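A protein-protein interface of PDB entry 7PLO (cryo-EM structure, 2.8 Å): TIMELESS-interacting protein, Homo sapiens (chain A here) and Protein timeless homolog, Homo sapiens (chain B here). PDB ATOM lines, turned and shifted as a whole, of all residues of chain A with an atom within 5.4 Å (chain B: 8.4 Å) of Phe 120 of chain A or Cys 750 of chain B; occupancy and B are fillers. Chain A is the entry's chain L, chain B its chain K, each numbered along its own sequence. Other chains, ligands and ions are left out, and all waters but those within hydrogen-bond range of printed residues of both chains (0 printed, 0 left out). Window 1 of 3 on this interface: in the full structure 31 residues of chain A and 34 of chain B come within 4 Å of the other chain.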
ATOM      1  N   ILE A 104      22.477  -2.134  19.580  1.00  0.00           N
ATOM      2  CA  ILE A 104      23.929  -2.101  19.460  1.00  0.00           C
ATOM      3  C   ILE A 104      24.402  -0.687  19.161  1.00  0.00           C
ATOM      4  O   ILE A 104      25.427  -0.245  19.692  1.00  0.00           O
ATOM      5  CB  ILE A 104      24.401  -3.105  18.387  1.00  0.00           C
ATOM      6  CG1 ILE A 104      24.195  -4.558  18.859  1.00  0.00           C
ATOM      7  CG2 ILE A 104      25.862  -2.856  17.989  1.00  0.00           C
ATOM      8  CD1 ILE A 104      25.113  -5.042  19.994  1.00  0.00           C
ATOM      9  N   MET A 107      24.157   1.300  22.503  1.00  0.00           N
ATOM     10  CA  MET A 107      25.196   0.877  23.441  1.00  0.00           C
ATOM     11  C   MET A 107      26.571   1.356  22.988  1.00  0.00           C
ATOM     12  O   MET A 107      27.377   1.823  23.805  1.00  0.00           O
ATOM     13  CB  MET A 107      25.196  -0.648  23.582  1.00  0.00           C
ATOM     14  CG  MET A 107      23.975  -1.255  24.277  1.00  0.00           C
ATOM     15  SD  MET A 107      23.654  -0.680  25.953  1.00  0.00           S
ATOM     16  CE  MET A 107      25.204  -1.031  26.776  1.00  0.00           C
ATOM     17  N   GLU A 108      26.852   1.248  21.688  1.00  0.00           N
ATOM     18  CA  GLU A 108      28.128   1.697  21.148  1.00  0.00           C
ATOM     19  C   GLU A 108      28.306   3.197  21.336  1.00  0.00           C
ATOM     20  O   GLU A 108      29.399   3.659  21.679  1.00  0.00           O
ATOM     21  CB  GLU A 108      28.204   1.324  19.668  1.00  0.00           C
ATOM     22  CG  GLU A 108      29.550   1.538  18.997  1.00  0.00           C
ATOM     23  CD  GLU A 108      29.430   1.558  17.492  1.00  0.00           C
ATOM     24  OE1 GLU A 108      29.016   0.534  16.908  1.00  0.00           O
ATOM     25  OE2 GLU A 108      29.728   2.609  16.891  1.00  0.00           O
ATOM     26  N   ALA A 111      29.094   3.886  24.992  1.00  0.00           N
ATOM     27  CA  ALA A 111      30.463   3.483  25.301  1.00  0.00           C
ATOM     28  C   ALA A 111      31.477   4.458  24.714  1.00  0.00           C
ATOM     29  O   ALA A 111      32.496   4.762  25.350  1.00  0.00           O
ATOM     30  CB  ALA A 111      30.718   2.071  24.778  1.00  0.00           C
ATOM     31  N   LEU A 118      38.932   3.366  23.029  1.00  0.00           N
ATOM     32  CA  LEU A 118      38.833   1.966  22.643  1.00  0.00           C
ATOM     33  C   LEU A 118      37.758   1.748  21.585  1.00  0.00           C
ATOM     34  O   LEU A 118      36.843   2.556  21.413  1.00  0.00           O
ATOM     35  CB  LEU A 118      38.511   1.094  23.859  1.00  0.00           C
ATOM     36  CG  LEU A 118      39.513   1.060  25.012  1.00  0.00           C
ATOM     37  CD1 LEU A 118      38.912   0.308  26.185  1.00  0.00           C
ATOM     38  CD2 LEU A 118      40.821   0.418  24.581  1.00  0.00           C
ATOM     39  N   GLN A 119      37.887   0.628  20.876  1.00  0.00           N
ATOM     40  CA  GLN A 119      36.803   0.111  20.060  1.00  0.00           C
ATOM     41  C   GLN A 119      35.765  -0.568  20.953  1.00  0.00           C
ATOM     42  O   GLN A 119      35.983  -0.795  22.146  1.00  0.00           O
ATOM     43  CB  GLN A 119      37.335  -0.861  19.006  1.00  0.00           C
ATOM     44  CG  GLN A 119      38.164  -0.200  17.912  1.00  0.00           C
ATOM     45  CD  GLN A 119      38.400  -1.115  16.724  1.00  0.00           C
ATOM     46  OE1 GLN A 119      38.040  -2.292  16.749  1.00  0.00           O
ATOM     47  NE2 GLN A 119      39.005  -0.574  15.672  1.00  0.00           N
ATOM     48  N   PHE A 120      34.617  -0.895  20.357  1.00  0.00           N
ATOM     49  CA  PHE A 120      33.464  -1.308  21.152  1.00  0.00           C
ATOM     50  C   PHE A 120      33.679  -2.675  21.797  1.00  0.00           C
ATOM     51  O   PHE A 120      33.359  -2.866  22.976  1.00  0.00           O
ATOM     52  CB  PHE A 120      32.211  -1.299  20.269  1.00  0.00           C
ATOM     53  CG  PHE A 120      30.912  -1.561  21.005  1.00  0.00           C
ATOM     54  CD1 PHE A 120      30.655  -1.010  22.253  1.00  0.00           C
ATOM     55  CD2 PHE A 120      29.925  -2.332  20.414  1.00  0.00           C
ATOM     56  CE1 PHE A 120      29.464  -1.250  22.904  1.00  0.00           C
ATOM     57  CE2 PHE A 120      28.727  -2.569  21.059  1.00  0.00           C
ATOM     58  CZ  PHE A 120      28.496  -2.023  22.303  1.00  0.00           C
ATOM     59  N   GLU A 121      34.232  -3.638  21.056  1.00  0.00           N
ATOM     60  CA  GLU A 121      34.441  -4.961  21.640  1.00  0.00           C
ATOM     61  C   GLU A 121      35.573  -4.959  22.661  1.00  0.00           C
ATOM     62  O   GLU A 121      35.508  -5.696  23.653  1.00  0.00           O
ATOM     63  CB  GLU A 121      34.708  -5.995  20.545  1.00  0.00           C
ATOM     64  CG  GLU A 121      33.449  -6.519  19.844  1.00  0.00           C
ATOM     65  CD  GLU A 121      32.992  -5.641  18.692  1.00  0.00           C
ATOM     66  OE1 GLU A 121      33.430  -4.475  18.609  1.00  0.00           O
ATOM     67  OE2 GLU A 121      32.192  -6.126  17.864  1.00  0.00           O
ATOM     68  N   ASP A 122      36.612  -4.147  22.448  1.00  0.00           N
ATOM     69  CA  ASP A 122      37.643  -3.993  23.471  1.00  0.00           C
ATOM     70  C   ASP A 122      37.054  -3.388  24.740  1.00  0.00           C
ATOM     71  O   ASP A 122      37.364  -3.829  25.857  1.00  0.00           O
ATOM     72  CB  ASP A 122      38.782  -3.122  22.940  1.00  0.00           C
ATOM     73  CG  ASP A 122      39.415  -3.690  21.683  1.00  0.00           C
ATOM     74  OD1 ASP A 122      39.305  -4.913  21.460  1.00  0.00           O
ATOM     75  OD2 ASP A 122      40.027  -2.913  20.920  1.00  0.00           O
ATOM     76  N   PHE A 123      36.187  -2.383  24.578  1.00  0.00           N
ATOM     77  CA  PHE A 123      35.477  -1.798  25.710  1.00  0.00           C
ATOM     78  C   PHE A 123      34.655  -2.851  26.444  1.00  0.00           C
ATOM     79  O   PHE A 123      34.622  -2.871  27.678  1.00  0.00           O
ATOM     80  CB  PHE A 123      34.586  -0.655  25.202  1.00  0.00           C
ATOM     81  CG  PHE A 123      33.646  -0.083  26.235  1.00  0.00           C
ATOM     82  CD1 PHE A 123      34.042   0.971  27.033  1.00  0.00           C
ATOM     83  CD2 PHE A 123      32.349  -0.566  26.370  1.00  0.00           C
ATOM     84  CE1 PHE A 123      33.183   1.509  27.971  1.00  0.00           C
ATOM     85  CE2 PHE A 123      31.492  -0.037  27.307  1.00  0.00           C
ATOM     86  CZ  PHE A 123      31.907   1.006  28.105  1.00  0.00           C
ATOM     87  N   ILE A 124      33.969  -3.718  25.698  1.00  0.00           N
ATOM     88  CA  ILE A 124      33.140  -4.748  26.321  1.00  0.00           C
ATOM     89  C   ILE A 124      34.009  -5.730  27.100  1.00  0.00           C
ATOM     90  O   ILE A 124      33.686  -6.111  28.234  1.00  0.00           O
ATOM     91  CB  ILE A 124      32.289  -5.470  25.259  1.00  0.00           C
ATOM     92  CG1 ILE A 124      31.218  -4.528  24.701  1.00  0.00           C
ATOM     93  CG2 ILE A 124      31.630  -6.724  25.852  1.00  0.00           C
ATOM     94  CD1 ILE A 124      30.668  -4.947  23.355  1.00  0.00           C
ATOM     95  N   ASP A 125      35.110  -6.177  26.494  1.00  0.00           N
ATOM     96  CA  ASP A 125      35.978  -7.140  27.161  1.00  0.00           C
ATOM     97  C   ASP A 125      36.625  -6.544  28.406  1.00  0.00           C
ATOM     98  O   ASP A 125      36.946  -7.280  29.346  1.00  0.00           O
ATOM     99  CB  ASP A 125      37.044  -7.645  26.188  1.00  0.00           C
ATOM    100  CG  ASP A 125      36.451  -8.418  25.022  1.00  0.00           C
ATOM    101  OD1 ASP A 125      35.222  -8.640  25.015  1.00  0.00           O
ATOM    102  OD2 ASP A 125      37.214  -8.803  24.112  1.00  0.00           O
ATOM    103  N   SER B 309      29.271   3.614  12.555  1.00  0.00           N
ATOM    104  CA  SER B 309      29.733   3.186  13.865  1.00  0.00           C
ATOM    105  C   SER B 309      30.880   4.096  14.275  1.00  0.00           C
ATOM    106  O   SER B 309      31.643   4.573  13.431  1.00  0.00           O
ATOM    107  CB  SER B 309      30.178   1.720  13.865  1.00  0.00           C
ATOM    108  OG  SER B 309      31.264   1.516  12.981  1.00  0.00           O
ATOM    109  N   SER B 310      30.996   4.338  15.583  1.00  0.00           N
ATOM    110  CA  SER B 310      32.012   5.255  16.089  1.00  0.00           C
ATOM    111  C   SER B 310      33.434   4.725  15.925  1.00  0.00           C
ATOM    112  O   SER B 310      34.381   5.511  16.037  1.00  0.00           O
ATOM    113  CB  SER B 310      31.751   5.561  17.564  1.00  0.00           C
ATOM    114  OG  SER B 310      30.500   6.205  17.735  1.00  0.00           O
ATOM    115  N   ASP B 311      33.608   3.426  15.665  1.00  0.00           N
ATOM    116  CA  ASP B 311      34.925   2.809  15.523  1.00  0.00           C
ATOM    117  C   ASP B 311      35.353   2.681  14.062  1.00  0.00           C
ATOM    118  O   ASP B 311      36.130   1.784  13.719  1.00  0.00           O
ATOM    119  CB  ASP B 311      34.952   1.442  16.215  1.00  0.00           C
ATOM    120  CG  ASP B 311      33.899   0.477  15.683  1.00  0.00           C
ATOM    121  OD1 ASP B 311      33.131   0.855  14.774  1.00  0.00           O
ATOM    122  OD2 ASP B 311      33.833  -0.662  16.190  1.00  0.00           O
ATOM    123  N   LYS B 314      39.181   4.021  14.203  1.00  0.00           N
ATOM    124  CA  LYS B 314      39.978   3.738  15.390  1.00  0.00           C
ATOM    125  C   LYS B 314      40.980   2.622  15.129  1.00  0.00           C
ATOM    126  O   LYS B 314      40.677   1.641  14.445  1.00  0.00           O
ATOM    127  CB  LYS B 314      39.078   3.342  16.558  1.00  0.00           C
ATOM    128  CG  LYS B 314      38.241   4.470  17.112  1.00  0.00           C
ATOM    129  CD  LYS B 314      37.436   3.987  18.294  1.00  0.00           C
ATOM    130  CE  LYS B 314      36.566   5.077  18.869  1.00  0.00           C
ATOM    131  NZ  LYS B 314      35.733   4.535  19.969  1.00  0.00           N
ATOM    132  N   ARG B 713      32.105 -17.821  18.550  1.00  0.00           N
ATOM    133  CA  ARG B 713      32.581 -16.668  17.782  1.00  0.00           C
ATOM    134  C   ARG B 713      33.157 -17.069  16.429  1.00  0.00           C
ATOM    135  O   ARG B 713      33.062 -16.300  15.466  1.00  0.00           O
ATOM    136  CB  ARG B 713      33.636 -15.900  18.576  1.00  0.00           C
ATOM    137  CG  ARG B 713      33.064 -15.060  19.691  1.00  0.00           C
ATOM    138  CD  ARG B 713      34.152 -14.385  20.496  1.00  0.00           C
ATOM    139  NE  ARG B 713      33.630 -13.869  21.756  1.00  0.00           N
ATOM    140  CZ  ARG B 713      34.363 -13.341  22.729  1.00  0.00           C
ATOM    141  NH1 ARG B 713      35.679 -13.220  22.627  1.00  0.00           N
ATOM    142  NH2 ARG B 713      33.759 -12.926  23.839  1.00  0.00           N
ATOM    143  N   TYR B 715      32.029 -19.365  14.390  1.00  0.00           N
ATOM    144  CA  TYR B 715      31.023 -20.184  13.716  1.00  0.00           C
ATOM    145  C   TYR B 715      31.262 -20.263  12.213  1.00  0.00           C
ATOM    146  O   TYR B 715      30.887 -21.254  11.577  1.00  0.00           O
ATOM    147  CB  TYR B 715      29.621 -19.630  13.991  1.00  0.00           C
ATOM    148  CG  TYR B 715      29.311 -18.327  13.280  1.00  0.00           C
ATOM    149  CD1 TYR B 715      29.733 -17.111  13.798  1.00  0.00           C
ATOM    150  CD2 TYR B 715      28.593 -18.316  12.089  1.00  0.00           C
ATOM    151  CE1 TYR B 715      29.453 -15.923  13.150  1.00  0.00           C
ATOM    152  CE2 TYR B 715      28.311 -17.136  11.435  1.00  0.00           C
ATOM    153  CZ  TYR B 715      28.742 -15.942  11.969  1.00  0.00           C
ATOM    154  OH  TYR B 715      28.460 -14.764  11.319  1.00  0.00           O
ATOM    155  N   GLN B 745      23.707 -11.220  27.251  1.00  0.00           N
ATOM    156  CA  GLN B 745      24.976 -10.527  27.441  1.00  0.00           C
ATOM    157  C   GLN B 745      25.289  -9.652  26.238  1.00  0.00           C
ATOM    158  O   GLN B 745      24.837  -9.912  25.121  1.00  0.00           O
ATOM    159  CB  GLN B 745      26.129 -11.509  27.663  1.00  0.00           C
ATOM    160  CG  GLN B 745      26.168 -12.140  29.040  1.00  0.00           C
ATOM    161  CD  GLN B 745      26.523 -11.147  30.126  1.00  0.00           C
ATOM    162  OE1 GLN B 745      27.691 -10.818  30.328  1.00  0.00           O
ATOM    163  NE2 GLN B 745      25.509 -10.653  30.827  1.00  0.00           N
ATOM    164  N   LEU B 746      26.087  -8.612  26.486  1.00  0.00           N
ATOM    165  CA  LEU B 746      26.376  -7.629  25.447  1.00  0.00           C
ATOM    166  C   LEU B 746      27.335  -8.184  24.400  1.00  0.00           C
ATOM    167  O   LEU B 746      27.133  -7.974  23.199  1.00  0.00           O
ATOM    168  CB  LEU B 746      26.942  -6.359  26.086  1.00  0.00           C
ATOM    169  CG  LEU B 746      27.229  -5.151  25.190  1.00  0.00           C
ATOM    170  CD1 LEU B 746      26.010  -4.731  24.380  1.00  0.00           C
ATOM    171  CD2 LEU B 746      27.713  -3.994  26.046  1.00  0.00           C
ATOM    172  N   SER B 747      28.392  -8.877  24.831  1.00  0.00           N
ATOM    173  CA  SER B 747      29.305  -9.504  23.876  1.00  0.00           C
ATOM    174  C   SER B 747      28.594 -10.585  23.069  1.00  0.00           C
ATOM    175  O   SER B 747      28.790 -10.703  21.848  1.00  0.00           O
ATOM    176  CB  SER B 747      30.508 -10.089  24.614  1.00  0.00           C
ATOM    177  OG  SER B 747      30.103 -10.875  25.721  1.00  0.00           O
ATOM    178  N   VAL B 748      27.757 -11.378  23.737  1.00  0.00           N
ATOM    179  CA  VAL B 748      26.981 -12.401  23.043  1.00  0.00           C
ATOM    180  C   VAL B 748      26.019 -11.742  22.062  1.00  0.00           C
ATOM    181  O   VAL B 748      25.756 -12.270  20.976  1.00  0.00           O
ATOM    182  CB  VAL B 748      26.248 -13.300  24.064  1.00  0.00           C
ATOM    183  CG1 VAL B 748      25.387 -14.343  23.365  1.00  0.00           C
ATOM    184  CG2 VAL B 748      27.240 -14.018  25.003  1.00  0.00           C
ATOM    185  N   PHE B 749      25.486 -10.572  22.423  1.00  0.00           N
ATOM    186  CA  PHE B 749      24.608  -9.846  21.511  1.00  0.00           C
ATOM    187  C   PHE B 749      25.371  -9.264  20.328  1.00  0.00           C
ATOM    188  O   PHE B 749      24.815  -9.172  19.232  1.00  0.00           O
ATOM    189  CB  PHE B 749      23.865  -8.738  22.266  1.00  0.00           C
ATOM    190  CG  PHE B 749      22.611  -9.196  22.992  1.00  0.00           C
ATOM    191  CD1 PHE B 749      22.422 -10.519  23.388  1.00  0.00           C
ATOM    192  CD2 PHE B 749      21.616  -8.280  23.279  1.00  0.00           C
ATOM    193  CE1 PHE B 749      21.271 -10.905  24.042  1.00  0.00           C
ATOM    194  CE2 PHE B 749      20.467  -8.666  23.934  1.00  0.00           C
ATOM    195  CZ  PHE B 749      20.294  -9.978  24.317  1.00  0.00           C
ATOM    196  N   CYS B 750      26.631  -8.867  20.514  1.00  0.00           N
ATOM    197  CA  CYS B 750      27.446  -8.472  19.367  1.00  0.00           C
ATOM    198  C   CYS B 750      27.664  -9.650  18.426  1.00  0.00           C
ATOM    199  O   CYS B 750      27.611  -9.503  17.195  1.00  0.00           O
ATOM    200  CB  CYS B 750      28.787  -7.913  19.841  1.00  0.00           C
ATOM    201  SG  CYS B 750      28.688  -6.279  20.602  1.00  0.00           S
ATOM    202  N   LEU B 751      27.912 -10.833  18.991  1.00  0.00           N
ATOM    203  CA  LEU B 751      28.048 -12.023  18.158  1.00  0.00           C
ATOM    204  C   LEU B 751      26.749 -12.331  17.419  1.00  0.00           C
ATOM    205  O   LEU B 751      26.767 -12.701  16.237  1.00  0.00           O
ATOM    206  CB  LEU B 751      28.487 -13.212  19.014  1.00  0.00           C
ATOM    207  CG  LEU B 751      28.657 -14.572  18.328  1.00  0.00           C
ATOM    208  CD1 LEU B 751      29.531 -14.493  17.080  1.00  0.00           C
ATOM    209  CD2 LEU B 751      29.246 -15.562  19.318  1.00  0.00           C
ATOM    210  N   PHE B 752      25.607 -12.177  18.095  1.00  0.00           N
ATOM    211  CA  PHE B 752      24.320 -12.351  17.424  1.00  0.00           C
ATOM    212  C   PHE B 752      24.119 -11.307  16.334  1.00  0.00           C
ATOM    213  O   PHE B 752      23.505 -11.592  15.301  1.00  0.00           O
ATOM    214  CB  PHE B 752      23.166 -12.268  18.433  1.00  0.00           C
ATOM    215  CG  PHE B 752      23.087 -13.416  19.428  1.00  0.00           C
ATOM    216  CD1 PHE B 752      23.729 -14.635  19.225  1.00  0.00           C
ATOM    217  CD2 PHE B 752      22.328 -13.263  20.574  1.00  0.00           C
ATOM    218  CE1 PHE B 752      23.623 -15.654  20.147  1.00  0.00           C
ATOM    219  CE2 PHE B 752      22.219 -14.279  21.495  1.00  0.00           C
ATOM    220  CZ  PHE B 752      22.867 -15.477  21.283  1.00  0.00           C
ATOM    221  N   ASN B 753      24.597 -10.082  16.559  1.00  0.00           N
ATOM    222  CA  ASN B 753      24.503  -9.047  15.534  1.00  0.00           C
ATOM    223  C   ASN B 753      25.269  -9.457  14.285  1.00  0.00           C
ATOM    224  O   ASN B 753      24.769  -9.313  13.161  1.00  0.00           O
ATOM    225  CB  ASN B 753      25.033  -7.724  16.085  1.00  0.00           C
ATOM    226  CG  ASN B 753      24.910  -6.587  15.095  1.00  0.00           C
ATOM    227  OD1 ASN B 753      24.000  -6.562  14.269  1.00  0.00           O
ATOM    228  ND2 ASN B 753      25.835  -5.635  15.173  1.00  0.00           N
ATOM    229  N   ARG B 754      26.474 -10.001  14.468  1.00  0.00           N
ATOM    230  CA  ARG B 754      27.226 -10.522  13.328  1.00  0.00           C
ATOM    231  C   ARG B 754      26.487 -11.673  12.652  1.00  0.00           C
ATOM    232  O   ARG B 754      26.445 -11.755  11.418  1.00  0.00           O
ATOM    233  CB  ARG B 754      28.616 -10.977  13.771  1.00  0.00           C
ATOM    234  CG  ARG B 754      29.605  -9.840  13.949  1.00  0.00           C
ATOM    235  CD  ARG B 754      31.013 -10.341  14.240  1.00  0.00           C
ATOM    236  NE  ARG B 754      31.335 -10.285  15.661  1.00  0.00           N
ATOM    237  CZ  ARG B 754      31.636  -9.181  16.333  1.00  0.00           C
ATOM    238  NH1 ARG B 754      31.626  -7.986  15.758  1.00  0.00           N
ATOM    239  NH2 ARG B 754      31.951  -9.273  17.622  1.00  0.00           N
ATOM    240  N   LEU B 755      25.902 -12.575  13.449  1.00  0.00           N
ATOM    241  CA  LEU B 755      25.168 -13.708  12.885  1.00  0.00           C
ATOM    242  C   LEU B 755      23.991 -13.244  12.036  1.00  0.00           C
ATOM    243  O   LEU B 755      23.768 -13.761  10.934  1.00  0.00           O
ATOM    244  CB  LEU B 755      24.673 -14.631  14.001  1.00  0.00           C
ATOM    245  CG  LEU B 755      25.514 -15.873  14.296  1.00  0.00           C
ATOM    246  CD1 LEU B 755      25.189 -16.425  15.676  1.00  0.00           C
ATOM    247  CD2 LEU B 755      25.283 -16.936  13.233  1.00  0.00           C
ATOM    248  N   LEU B 756      23.226 -12.273  12.533  1.00  0.00           N
ATOM    249  CA  LEU B 756      22.084 -11.773  11.775  1.00  0.00           C
ATOM    250  C   LEU B 756      22.527 -10.990  10.546  1.00  0.00           C
ATOM    251  O   LEU B 756      21.844 -11.027   9.515  1.00  0.00           O
ATOM    252  CB  LEU B 756      21.188 -10.901  12.664  1.00  0.00           C
ATOM    253  CG  LEU B 756      20.074 -11.551  13.506  1.00  0.00           C
ATOM    254  CD1 LEU B 756      19.024 -12.241  12.638  1.00  0.00           C
ATOM    255  CD2 LEU B 756      20.618 -12.521  14.547  1.00  0.00           C
ATOM    256  N   SER B 757      23.656 -10.283  10.625  1.00  0.00           N
ATOM    257  CA  SER B 757      24.156  -9.511   9.494  1.00  0.00           C
ATOM    258  C   SER B 757      24.952 -10.342   8.492  1.00  0.00           C
ATOM    259  O   SER B 757      25.363  -9.797   7.462  1.00  0.00           O
ATOM    260  CB  SER B 757      25.032  -8.361   9.998  1.00  0.00           C
ATOM    261  OG  SER B 757      24.342  -7.571  10.950  1.00  0.00           O
ATOM    262  N   LEU B 775      16.759 -13.388  21.533  1.00  0.00           N
ATOM    263  CA  LEU B 775      16.587 -11.947  21.376  1.00  0.00           C
ATOM    264  C   LEU B 775      15.142 -11.531  21.615  1.00  0.00           C
ATOM    265  O   LEU B 775      14.888 -10.497  22.242  1.00  0.00           O
ATOM    266  CB  LEU B 775      17.044 -11.513  19.983  1.00  0.00           C
ATOM    267  CG  LEU B 775      18.555 -11.494  19.730  1.00  0.00           C
ATOM    268  CD1 LEU B 775      18.842 -11.464  18.235  1.00  0.00           C
ATOM    269  CD2 LEU B 775      19.214 -10.311  20.421  1.00  0.00           C
ATOM    270  N   LEU B 792      22.699  -6.333  30.740  1.00  0.00           N
ATOM    271  CA  LEU B 792      23.487  -6.889  29.639  1.00  0.00           C
ATOM    272  C   LEU B 792      24.991  -6.704  29.828  1.00  0.00           C
ATOM    273  O   LEU B 792      25.772  -7.470  29.252  1.00  0.00           O
ATOM    274  CB  LEU B 792      23.095  -6.242  28.308  1.00  0.00           C
ATOM    275  CG  LEU B 792      21.805  -6.634  27.586  1.00  0.00           C
ATOM    276  CD1 LEU B 792      21.703  -5.823  26.301  1.00  0.00           C
ATOM    277  CD2 LEU B 792      21.742  -8.122  27.276  1.00  0.00           C
ATOM    278  N   LEU B 793      25.415  -5.713  30.612  1.00  0.00           N
ATOM    279  CA  LEU B 793      26.796  -5.251  30.576  1.00  0.00           C
ATOM    280  C   LEU B 793      27.780  -6.164  31.307  1.00  0.00           C
ATOM    281  O   LEU B 793      28.986  -6.041  31.065  1.00  0.00           O
ATOM    282  CB  LEU B 793      26.860  -3.836  31.167  1.00  0.00           C
ATOM    283  CG  LEU B 793      28.096  -2.960  30.934  1.00  0.00           C
ATOM    284  CD1 LEU B 793      28.325  -2.674  29.458  1.00  0.00           C
ATOM    285  CD2 LEU B 793      27.945  -1.650  31.693  1.00  0.00           C
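Of the 22 printed residues of chain B, 9 touch a printed residue of chain A.
Hydrophobic or aromatic side chains of chain B within 4 Å of the printed part of chain A: Leu 746.
Hydrophobic or aromatic side chains of chain A that line the printed part of chain B: Ile 104, Met 107, Phe 120 and Ile 124.
Among the printed residues, 13 pairs touch across the chains.
Among the printed residues, Asp or Glu carboxylates within 4 Å of a Lys or Arg side-chain nitrogen of the other chain: Glu 121 of chain A with Arg 754 of chain B.
The backbone NH (N) of Ser 310 of chain B sits at hydrogen-bond distance from the side-chain carboxylate (OE2) of Glu 108 of chain A, at 2.5 Å.
NZ of Lys 314 of chain B is in hydrogen-bond range of O of Leu 118 of chain A, 2.7 Å away.
The backbone carbonyl oxygen (O) of Lys 314 of chain B lies within hydrogen-bond range of the side-chain amide nitrogen (NE2) of Gln 119 of chain A, at 3.0 Å.
The guanidinium group (NH1) of Arg 754 of chain B is in salt-bridge range of the side-chain carboxylate (OE2) of Glu 121 of chain A, at 2.9 Å.
The side-chain hydroxyl (OG) of Ser 309 of chain B sits at hydrogen-bond distance from the side-chain carboxylate (OD1) of Asp 311 of chain B, 2.7 Å away.
SG of Cys 750 of chain B is in hydrogen-bond range of O of Leu 746 of chain B (3.5 Å).
N of Leu 746 of chain B sits at hydrogen-bond distance from O of Leu 792 of chain B, at 3.0 Å.
O of Asn 753 of chain B sits at hydrogen-bond distance from OG of Ser 757 of chain B.
Among the printed residues, merely in contact across the chains: Glu 108 of chain A with Ser 309 of chain B (3.1 Å), Ile 124 of chain A with Cys 750 of chain B (3.6 Å), Phe 120 of chain A with Cys 750 of chain B (3.7 Å), Ile 124 of chain A with Ser 747 of chain B (3.8 Å), Ile 124 of chain A with Leu 746 of chain B (3.8 Å), Ile 104 of chain A with Cys 750 of chain B (3.8 Å), Met 107 of chain A with Leu 746 of chain B (3.95 Å), Ile 104 of chain A with Asn 753 of chain B (3.96 Å) and Gln 119 of chain A with Asp 311 of chain B (3.99 Å).
Of the printed residues of chain B, Met 107 of chain A touches Leu 746.
Printed residues of chain B within 4 Å of Leu 118 of chain A: Lys 314.
Printed residues of chain B within 4 Å of Ile 124 of chain A: Leu 746, Ser 747 and Cys 750.
Asp 125 of chain A touches none of the printed residues of chain B.
Gln 745 of chain B touches none of the printed residues of chain A.
Printed residues of chain A within 4 Å of Leu 746 of chain B: Met 107 and Ile 124.
Cys 750 of chain B touches three residues of chain A.
The nearest residue of chain A that does not touch Cys 750 of chain B is Glu 121 of chain A (4.3 Å).
The nearest printed residue of chain B that does not touch Met 107 of chain A is Leu 793 of chain B (4.4 Å).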
